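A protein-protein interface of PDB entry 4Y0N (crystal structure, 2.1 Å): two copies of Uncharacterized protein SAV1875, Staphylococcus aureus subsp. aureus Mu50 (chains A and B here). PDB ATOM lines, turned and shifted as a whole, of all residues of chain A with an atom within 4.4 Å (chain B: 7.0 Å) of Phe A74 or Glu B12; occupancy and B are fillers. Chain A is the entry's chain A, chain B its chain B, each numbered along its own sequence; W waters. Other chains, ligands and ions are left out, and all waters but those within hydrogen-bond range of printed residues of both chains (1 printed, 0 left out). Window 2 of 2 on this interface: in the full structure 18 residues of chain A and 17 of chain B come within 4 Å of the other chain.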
ATOM      1  N   ASN A  11     -24.486  22.348  27.647  1.00  0.00           N
ATOM      2  CA  ASN A  11     -23.133  21.836  27.431  1.00  0.00           C
ATOM      3  C   ASN A  11     -22.097  22.475  28.357  1.00  0.00           C
ATOM      4  O   ASN A  11     -22.223  23.640  28.734  1.00  0.00           O
ATOM      5  CB  ASN A  11     -22.733  22.027  25.965  1.00  0.00           C
ATOM      6  CG  ASN A  11     -23.457  21.071  25.042  1.00  0.00           C
ATOM      7  OD1 ASN A  11     -23.464  19.866  25.283  1.00  0.00           O
ATOM      8  ND2 ASN A  11     -24.225  21.615  24.111  1.00  0.00           N
ATOM      9  N   GLU A  12     -21.072  21.710  28.717  1.00  0.00           N
ATOM     10  CA  GLU A  12     -19.917  22.237  29.437  1.00  0.00           C
ATOM     11  C   GLU A  12     -20.237  22.622  30.889  1.00  0.00           C
ATOM     12  O   GLU A  12     -19.505  23.394  31.507  1.00  0.00           O
ATOM     13  CB  GLU A  12     -19.288  23.413  28.682  1.00  0.00           C
ATOM     14  CG  GLU A  12     -18.873  23.055  27.255  1.00  0.00           C
ATOM     15  CD  GLU A  12     -18.025  24.135  26.607  1.00  0.00           C
ATOM     16  OE1 GLU A  12     -18.595  25.128  26.128  1.00  0.00           O
ATOM     17  OE2 GLU A  12     -16.785  24.045  26.685  1.00  0.00           O
ATOM     18  N   LYS A  46     -17.785  19.320  30.800  1.00  0.00           N
ATOM     19  CA  LYS A  46     -16.397  19.654  30.517  1.00  0.00           C
ATOM     20  C   LYS A  46     -15.497  18.446  30.410  1.00  0.00           C
ATOM     21  O   LYS A  46     -14.515  18.476  29.673  1.00  0.00           O
ATOM     22  CB  LYS A  46     -15.842  20.611  31.566  1.00  0.00           C
ATOM     23  CG  LYS A  46     -16.337  22.032  31.385  1.00  0.00           C
ATOM     24  CD  LYS A  46     -16.057  22.859  32.621  1.00  0.00           C
ATOM     25  CE  LYS A  46     -14.861  23.761  32.379  1.00  0.00           C
ATOM     26  NZ  LYS A  46     -15.235  25.152  32.739  1.00  0.00           N
ATOM     27  N   GLY A  72     -22.455  24.525  37.860  1.00  0.00           N
ATOM     28  CA  GLY A  72     -21.573  25.529  37.254  1.00  0.00           C
ATOM     29  C   GLY A  72     -20.806  25.021  36.031  1.00  0.00           C
ATOM     30  O   GLY A  72     -21.385  24.381  35.140  1.00  0.00           O
ATOM     31  N   GLY A  73     -19.521  25.350  35.951  1.00  0.00           N
ATOM     32  CA  GLY A  73     -18.816  25.290  34.670  1.00  0.00           C
ATOM     33  C   GLY A  73     -19.313  26.385  33.735  1.00  0.00           C
ATOM     34  O   GLY A  73     -19.654  27.469  34.183  1.00  0.00           O
ATOM     35  N   PHE A  74     -19.335  26.109  32.434  1.00  0.00           N
ATOM     36  CA  PHE A  74     -19.804  27.098  31.480  1.00  0.00           C
ATOM     37  C   PHE A  74     -21.249  26.860  31.038  1.00  0.00           C
ATOM     38  O   PHE A  74     -21.737  27.519  30.115  1.00  0.00           O
ATOM     39  CB  PHE A  74     -18.871  27.167  30.278  1.00  0.00           C
ATOM     40  CG  PHE A  74     -17.473  27.592  30.634  1.00  0.00           C
ATOM     41  CD1 PHE A  74     -17.257  28.742  31.372  1.00  0.00           C
ATOM     42  CD2 PHE A  74     -16.380  26.849  30.220  1.00  0.00           C
ATOM     43  CE1 PHE A  74     -15.976  29.142  31.710  1.00  0.00           C
ATOM     44  CE2 PHE A  74     -15.098  27.222  30.579  1.00  0.00           C
ATOM     45  CZ  PHE A  74     -14.892  28.373  31.325  1.00  0.00           C
ATOM     46  N   SER A  75     -21.928  25.917  31.699  1.00  0.00           N
ATOM     47  CA  SER A  75     -23.334  25.644  31.411  1.00  0.00           C
ATOM     48  C   SER A  75     -24.221  26.874  31.633  1.00  0.00           C
ATOM     49  O   SER A  75     -24.967  27.264  30.733  1.00  0.00           O
ATOM     50  CB  SER A  75     -23.828  24.434  32.203  1.00  0.00           C
ATOM     51  OG  SER A  75     -25.242  24.352  32.196  1.00  0.00           O
ATOM     52  N   PRO A  76     -24.034  27.578  32.756  1.00  0.00           N
ATOM     53  CA  PRO A  76     -24.816  28.794  33.010  1.00  0.00           C
ATOM     54  C   PRO A  76     -24.598  29.897  31.967  1.00  0.00           C
ATOM     55  O   PRO A  76     -25.571  30.504  31.492  1.00  0.00           O
ATOM     56  CB  PRO A  76     -24.312  29.249  34.387  1.00  0.00           C
ATOM     57  CG  PRO A  76     -23.921  27.967  35.054  1.00  0.00           C
ATOM     58  CD  PRO A  76     -23.283  27.152  33.952  1.00  0.00           C
ATOM     59  N   ASP A  77     -23.359  30.059  31.511  1.00  0.00           N
ATOM     60  CA  ASP A  77     -23.072  31.012  30.440  1.00  0.00           C
ATOM     61  C   ASP A  77     -23.775  30.615  29.129  1.00  0.00           C
ATOM     62  O   ASP A  77     -24.499  31.420  28.544  1.00  0.00           O
ATOM     63  CB  ASP A  77     -21.555  31.167  30.245  1.00  0.00           C
ATOM     64  CG  ASP A  77     -21.195  32.336  29.325  1.00  0.00           C
ATOM     65  OD1 ASP A  77     -20.623  33.332  29.821  1.00  0.00           O
ATOM     66  OD2 ASP A  77     -21.326  32.189  28.095  1.00  0.00           O
ATOM     67  N   HIS A  78     -23.714  29.334  28.767  1.00  0.00           N
ATOM     68  CA  HIS A  78     -24.504  28.838  27.640  1.00  0.00           C
ATOM     69  C   HIS A  78     -25.994  29.109  27.766  1.00  0.00           C
ATOM     70  O   HIS A  78     -26.608  29.671  26.844  1.00  0.00           O
ATOM     71  CB  HIS A  78     -24.242  27.357  27.393  1.00  0.00           C
ATOM     72  CG  HIS A  78     -22.890  27.077  26.776  1.00  0.00           C
ATOM     73  ND1 HIS A  78     -22.493  27.641  25.616  1.00  0.00           N
ATOM     74  CD2 HIS A  78     -21.850  26.246  27.188  1.00  0.00           C
ATOM     75  CE1 HIS A  78     -21.294  27.145  25.263  1.00  0.00           C
ATOM     76  NE2 HIS A  78     -20.876  26.329  26.252  1.00  0.00           N
ATOM     77  N   LEU B   9      -4.691  36.772  27.255  1.00  0.00           N
ATOM     78  CA  LEU B   9      -5.153  35.498  26.728  1.00  0.00           C
ATOM     79  C   LEU B   9      -5.016  34.391  27.780  1.00  0.00           C
ATOM     80  O   LEU B   9      -4.003  34.309  28.484  1.00  0.00           O
ATOM     81  CB  LEU B   9      -4.360  35.141  25.467  1.00  0.00           C
ATOM     82  CG  LEU B   9      -5.063  34.311  24.390  1.00  0.00           C
ATOM     83  CD1 LEU B   9      -6.318  35.005  23.878  1.00  0.00           C
ATOM     84  CD2 LEU B   9      -4.098  34.043  23.243  1.00  0.00           C
ATOM     85  N   ALA B  10      -6.092  33.639  27.973  1.00  0.00           N
ATOM     86  CA  ALA B  10      -6.042  32.369  28.695  1.00  0.00           C
ATOM     87  C   ALA B  10      -6.550  31.244  27.786  1.00  0.00           C
ATOM     88  O   ALA B  10      -6.797  31.459  26.593  1.00  0.00           O
ATOM     89  CB  ALA B  10      -6.871  32.442  29.969  1.00  0.00           C
ATOM     90  N   ASN B  11      -6.683  30.041  28.340  1.00  0.00           N
ATOM     91  CA  ASN B  11      -7.160  28.911  27.548  1.00  0.00           C
ATOM     92  C   ASN B  11      -8.591  29.148  27.096  1.00  0.00           C
ATOM     93  O   ASN B  11      -9.337  29.912  27.728  1.00  0.00           O
ATOM     94  CB  ASN B  11      -7.057  27.595  28.349  1.00  0.00           C
ATOM     95  CG  ASN B  11      -5.634  27.078  28.433  1.00  0.00           C
ATOM     96  OD1 ASN B  11      -4.967  26.887  27.419  1.00  0.00           O
ATOM     97  ND2 ASN B  11      -5.148  26.894  29.654  1.00  0.00           N
ATOM     98  N   GLU B  12      -8.976  28.493  26.005  1.00  0.00           N
ATOM     99  CA  GLU B  12     -10.364  28.494  25.562  1.00  0.00           C
ATOM    100  C   GLU B  12     -10.841  29.851  25.026  1.00  0.00           C
ATOM    101  O   GLU B  12     -12.052  30.112  24.985  1.00  0.00           O
ATOM    102  CB  GLU B  12     -11.287  28.033  26.703  1.00  0.00           C
ATOM    103  CG  GLU B  12     -10.938  26.647  27.245  1.00  0.00           C
ATOM    104  CD  GLU B  12     -12.039  26.065  28.116  1.00  0.00           C
ATOM    105  OE1 GLU B  12     -12.090  26.370  29.327  1.00  0.00           O
ATOM    106  OE2 GLU B  12     -12.929  25.409  27.559  1.00  0.00           O
ATOM    107  N   PHE B  13      -9.906  30.717  24.634  1.00  0.00           N
ATOM    108  CA  PHE B  13     -10.230  31.830  23.740  1.00  0.00           C
ATOM    109  C   PHE B  13     -10.879  31.295  22.463  1.00  0.00           C
ATOM    110  O   PHE B  13     -10.601  30.162  22.058  1.00  0.00           O
ATOM    111  CB  PHE B  13      -8.973  32.659  23.398  1.00  0.00           C
ATOM    112  CG  PHE B  13      -7.921  31.898  22.616  1.00  0.00           C
ATOM    113  CD1 PHE B  13      -6.890  31.233  23.274  1.00  0.00           C
ATOM    114  CD2 PHE B  13      -7.891  31.954  21.223  1.00  0.00           C
ATOM    115  CE1 PHE B  13      -5.915  30.548  22.562  1.00  0.00           C
ATOM    116  CE2 PHE B  13      -6.895  31.316  20.507  1.00  0.00           C
ATOM    117  CZ  PHE B  13      -5.932  30.565  21.175  1.00  0.00           C
ATOM    118  N   GLU B  14     -11.752  32.096  21.847  1.00  0.00           N
ATOM    119  CA  GLU B  14     -12.286  31.772  20.526  1.00  0.00           C
ATOM    120  C   GLU B  14     -11.254  32.039  19.429  1.00  0.00           C
ATOM    121  O   GLU B  14     -10.870  33.194  19.191  1.00  0.00           O
ATOM    122  CB  GLU B  14     -13.568  32.570  20.246  1.00  0.00           C
ATOM    123  CG  GLU B  14     -14.141  32.352  18.853  1.00  0.00           C
ATOM    124  CD  GLU B  14     -14.861  31.025  18.712  1.00  0.00           C
ATOM    125  OE1 GLU B  14     -15.597  30.649  19.633  1.00  0.00           O
ATOM    126  OE2 GLU B  14     -14.682  30.335  17.687  1.00  0.00           O
ATOM    127  N   ASP B  15     -10.758  30.968  18.809  1.00  0.00           N
ATOM    128  CA  ASP B  15      -9.556  31.055  17.972  1.00  0.00           C
ATOM    129  C   ASP B  15      -9.491  32.313  17.099  1.00  0.00           C
ATOM    130  O   ASP B  15      -8.525  33.074  17.203  1.00  0.00           O
ATOM    131  CB  ASP B  15      -9.336  29.786  17.132  1.00  0.00           C
ATOM    132  CG  ASP B  15      -9.362  28.503  17.966  1.00  0.00           C
ATOM    133  OD1 ASP B  15     -10.015  28.468  19.036  1.00  0.00           O
ATOM    134  OD2 ASP B  15      -8.774  27.505  17.518  1.00  0.00           O
ATOM    135  N   VAL B  43      -1.165  28.600  25.573  1.00  0.00           N
ATOM    136  CA  VAL B  43      -2.617  28.530  25.784  1.00  0.00           C
ATOM    137  C   VAL B  43      -3.309  28.042  24.514  1.00  0.00           C
ATOM    138  O   VAL B  43      -2.777  28.186  23.414  1.00  0.00           O
ATOM    139  CB  VAL B  43      -3.213  29.877  26.249  1.00  0.00           C
ATOM    140  CG1 VAL B  43      -2.848  30.158  27.700  1.00  0.00           C
ATOM    141  CG2 VAL B  43      -2.763  31.018  25.346  1.00  0.00           C
ATOM    142  N   VAL B  44      -4.412  27.324  24.692  1.00  0.00           N
ATOM    143  CA  VAL B  44      -5.040  26.597  23.595  1.00  0.00           C
ATOM    144  C   VAL B  44      -6.466  27.108  23.372  1.00  0.00           C
ATOM    145  O   VAL B  44      -7.284  27.130  24.295  1.00  0.00           O
ATOM    146  CB  VAL B  44      -5.061  25.075  23.879  1.00  0.00           C
ATOM    147  CG1 VAL B  44      -5.608  24.312  22.678  1.00  0.00           C
ATOM    148  CG2 VAL B  44      -3.665  24.576  24.240  1.00  0.00           C
ATOM    149  N   GLY B  45      -6.776  27.474  22.133  1.00  0.00           N
ATOM    150  CA  GLY B  45      -8.096  27.965  21.794  1.00  0.00           C
ATOM    151  C   GLY B  45      -9.176  26.910  21.974  1.00  0.00           C
ATOM    152  O   GLY B  45      -8.879  25.728  22.099  1.00  0.00           O
ATOM    153  N   LYS B  46     -10.430  27.325  21.824  1.00  0.00           N
ATOM    154  CA  LYS B  46     -11.565  26.406  21.847  1.00  0.00           C
ATOM    155  C   LYS B  46     -11.445  25.361  20.751  1.00  0.00           C
ATOM    156  O   LYS B  46     -11.934  24.249  20.891  1.00  0.00           O
ATOM    157  CB  LYS B  46     -12.881  27.173  21.666  1.00  0.00           C
ATOM    158  CG  LYS B  46     -13.451  27.720  22.952  1.00  0.00           C
ATOM    159  CD  LYS B  46     -14.610  28.661  22.665  1.00  0.00           C
ATOM    160  CE  LYS B  46     -15.943  27.966  22.902  1.00  0.00           C
ATOM    161  NZ  LYS B  46     -16.804  28.772  23.808  1.00  0.00           N
ATOM    162  N   HIS B  47     -10.846  25.742  19.632  1.00  0.00           N
ATOM    163  CA  HIS B  47     -10.733  24.835  18.495  1.00  0.00           C
ATOM    164  C   HIS B  47      -9.293  24.461  18.256  1.00  0.00           C
ATOM    165  O   HIS B  47      -8.928  24.016  17.176  1.00  0.00           O
ATOM    166  CB  HIS B  47     -11.371  25.453  17.251  1.00  0.00           C
ATOM    167  CG  HIS B  47     -12.754  26.027  17.501  1.00  0.00           C
ATOM    168  ND1 HIS B  47     -13.859  25.251  17.575  1.00  0.00           N
ATOM    169  CD2 HIS B  47     -13.157  27.314  17.857  1.00  0.00           C
ATOM    170  CE1 HIS B  47     -14.926  26.015  17.868  1.00  0.00           C
ATOM    171  NE2 HIS B  47     -14.493  27.278  18.057  1.00  0.00           N
ATOM    172  N   GLY B  72     -12.457  36.902  22.875  1.00  0.00           N
ATOM    173  CA  GLY B  72     -13.568  36.312  23.628  1.00  0.00           C
ATOM    174  C   GLY B  72     -13.443  34.797  23.733  1.00  0.00           C
ATOM    175  O   GLY B  72     -12.362  34.282  23.967  1.00  0.00           O
ATOM    176  N   GLY B  73     -14.566  34.093  23.645  1.00  0.00           N
ATOM    177  CA  GLY B  73     -14.665  32.730  24.159  1.00  0.00           C
ATOM    178  C   GLY B  73     -14.732  32.712  25.671  1.00  0.00           C
ATOM    179  O   GLY B  73     -15.244  33.640  26.293  1.00  0.00           O
ATOM    180  N   PHE B  74     -14.155  31.686  26.270  1.00  0.00           N
ATOM    181  CA  PHE B  74     -14.126  31.584  27.714  1.00  0.00           C
ATOM    182  C   PHE B  74     -12.779  32.022  28.290  1.00  0.00           C
ATOM    183  O   PHE B  74     -12.550  31.918  29.503  1.00  0.00           O
ATOM    184  CB  PHE B  74     -14.488  30.162  28.141  1.00  0.00           C
ATOM    185  CG  PHE B  74     -15.921  29.789  27.829  1.00  0.00           C
ATOM    186  CD1 PHE B  74     -16.970  30.630  28.199  1.00  0.00           C
ATOM    187  CD2 PHE B  74     -16.216  28.627  27.125  1.00  0.00           C
ATOM    188  CE1 PHE B  74     -18.295  30.298  27.907  1.00  0.00           C
ATOM    189  CE2 PHE B  74     -17.530  28.313  26.791  1.00  0.00           C
ATOM    190  CZ  PHE B  74     -18.572  29.146  27.190  1.00  0.00           C
ATOM    191  N   SER B  75     -11.957  32.659  27.449  1.00  0.00           N
ATOM    192  CA  SER B  75     -10.656  33.160  27.917  1.00  0.00           C
ATOM    193  C   SER B  75     -10.849  34.280  28.937  1.00  0.00           C
ATOM    194  O   SER B  75     -10.264  34.242  30.020  1.00  0.00           O
ATOM    195  CB  SER B  75      -9.782  33.636  26.753  1.00  0.00           C
ATOM    196  OG  SER B  75      -8.755  34.515  27.206  1.00  0.00           O
ATOM    197  N   PRO B  76     -11.768  35.218  28.648  1.00  0.00           N
ATOM    198  CA  PRO B  76     -11.945  36.298  29.612  1.00  0.00           C
ATOM    199  C   PRO B  76     -12.419  35.774  30.963  1.00  0.00           C
ATOM    200  O   PRO B  76     -11.890  36.176  32.001  1.00  0.00           O
ATOM    201  CB  PRO B  76     -12.986  37.196  28.934  1.00  0.00           C
ATOM    202  CG  PRO B  76     -12.710  37.002  27.466  1.00  0.00           C
ATOM    203  CD  PRO B  76     -12.394  35.529  27.349  1.00  0.00           C
ATOM    204  N   ASP B  77     -13.340  34.814  30.953  1.00  0.00           N
ATOM    205  CA  ASP B  77     -13.781  34.198  32.204  1.00  0.00           C
ATOM    206  C   ASP B  77     -12.616  33.582  32.999  1.00  0.00           C
ATOM    207  O   ASP B  77     -12.472  33.852  34.194  1.00  0.00           O
ATOM    208  CB  ASP B  77     -14.910  33.175  31.960  1.00  0.00           C
ATOM    209  CG  ASP B  77     -15.617  32.774  33.244  1.00  0.00           C
ATOM    210  OD1 ASP B  77     -16.738  33.247  33.509  1.00  0.00           O
ATOM    211  OD2 ASP B  77     -15.040  31.980  34.002  1.00  0.00           O
ATOM    212  N   HIS B  78     -11.753  32.812  32.337  1.00  0.00           N
ATOM    213  CA  HIS B  78     -10.564  32.273  33.017  1.00  0.00           C
ATOM    214  C   HIS B  78      -9.714  33.362  33.619  1.00  0.00           C
ATOM    215  O   HIS B  78      -9.232  33.232  34.751  1.00  0.00           O
ATOM    216  CB  HIS B  78      -9.708  31.415  32.079  1.00  0.00           C
ATOM    217  CG  HIS B  78     -10.305  30.058  31.765  1.00  0.00           C
ATOM    218  ND1 HIS B  78     -10.659  29.184  32.724  1.00  0.00           N
ATOM    219  CD2 HIS B  78     -10.550  29.424  30.546  1.00  0.00           C
ATOM    220  CE1 HIS B  78     -11.204  28.087  32.153  1.00  0.00           C
ATOM    221  NE2 HIS B  78     -11.109  28.223  30.817  1.00  0.00           N
HETATM  222  O   HOH W   1     -19.131  33.942  32.055  1.00  0.00           O
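Phe A74 touches just these residues of chain B: Glu B12 (3.4 Å), Phe B74 (3.6 Å), Asp B77 (3.8 Å) and His B78 (3.8 Å). Of the printed residues of chain B, Asp A77 touches Phe B74. Printed residues of chain B within 4 Å of His A78: Phe B74 (3.8 Å). Glu B12 touches one residue of chain A. The nearest residue of chain B that does not touch Phe A74 is Ser B75 (6.5 Å). The nearest residue of chain A that does not touch Glu B12 is Glu A12 (4.2 Å).
Glu A12 touches Phe B74, and with the chains exchanged Phe A74 touches Glu B12. Phe A74 touches its own counterpart, Phe B74. Phe A74 touches Asp B77, and with the chains exchanged Asp A77 touches Phe B74. Phe A74 touches His B78, and with the chains exchanged His A78 touches Phe B74.
Hydrophobic or aromatic side chains of chain B within 4 Å of the printed part of chain A: Phe B74 and His B78. Printed residues of chain A that touch a printed residue of chain B: Glu A12, Phe A74, Asp A77 and His A78. Among the printed residues, 7 pairs touch across the chains. Among the printed residues, no Asp or Glu carboxylate lies within 4 Å of a Lys or Arg side-chain nitrogen of the other chain.
The backbone carbonyl oxygen of Glu A12 lies within hydrogen-bond range of the backbone NH of Phe A74, 2.9 Å away. The side-chain carboxylate of Glu A12 is in hydrogen-bond range of a ring nitrogen (NE2) of His A78 (2.6 Å). The backbone NH (N) of Glu B12 sits at hydrogen-bond distance from the backbone carbonyl oxygen (O) of Val B44, at 2.8 Å. N of Phe B74 is in hydrogen-bond range of O of Glu B12, at 2.9 Å. A ring nitrogen (NE2) of His B78 sits at hydrogen-bond distance from the side-chain carboxylate (OE1) of Glu B12.
Among the printed residues, merely in contact across the chains: Phe A74 with Glu B12, Glu A12 with Phe B74, Phe A74 with Phe B74, Asp A77 with Phe B74, His A78 with Phe B74, Phe A74 with Asp B77 and Phe A74 with His B78.
Water W1 lies within hydrogen-bond range of OD1 of Asp A77 (2.8 Å) and OD1 of Asp B77 (2.9 Å).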
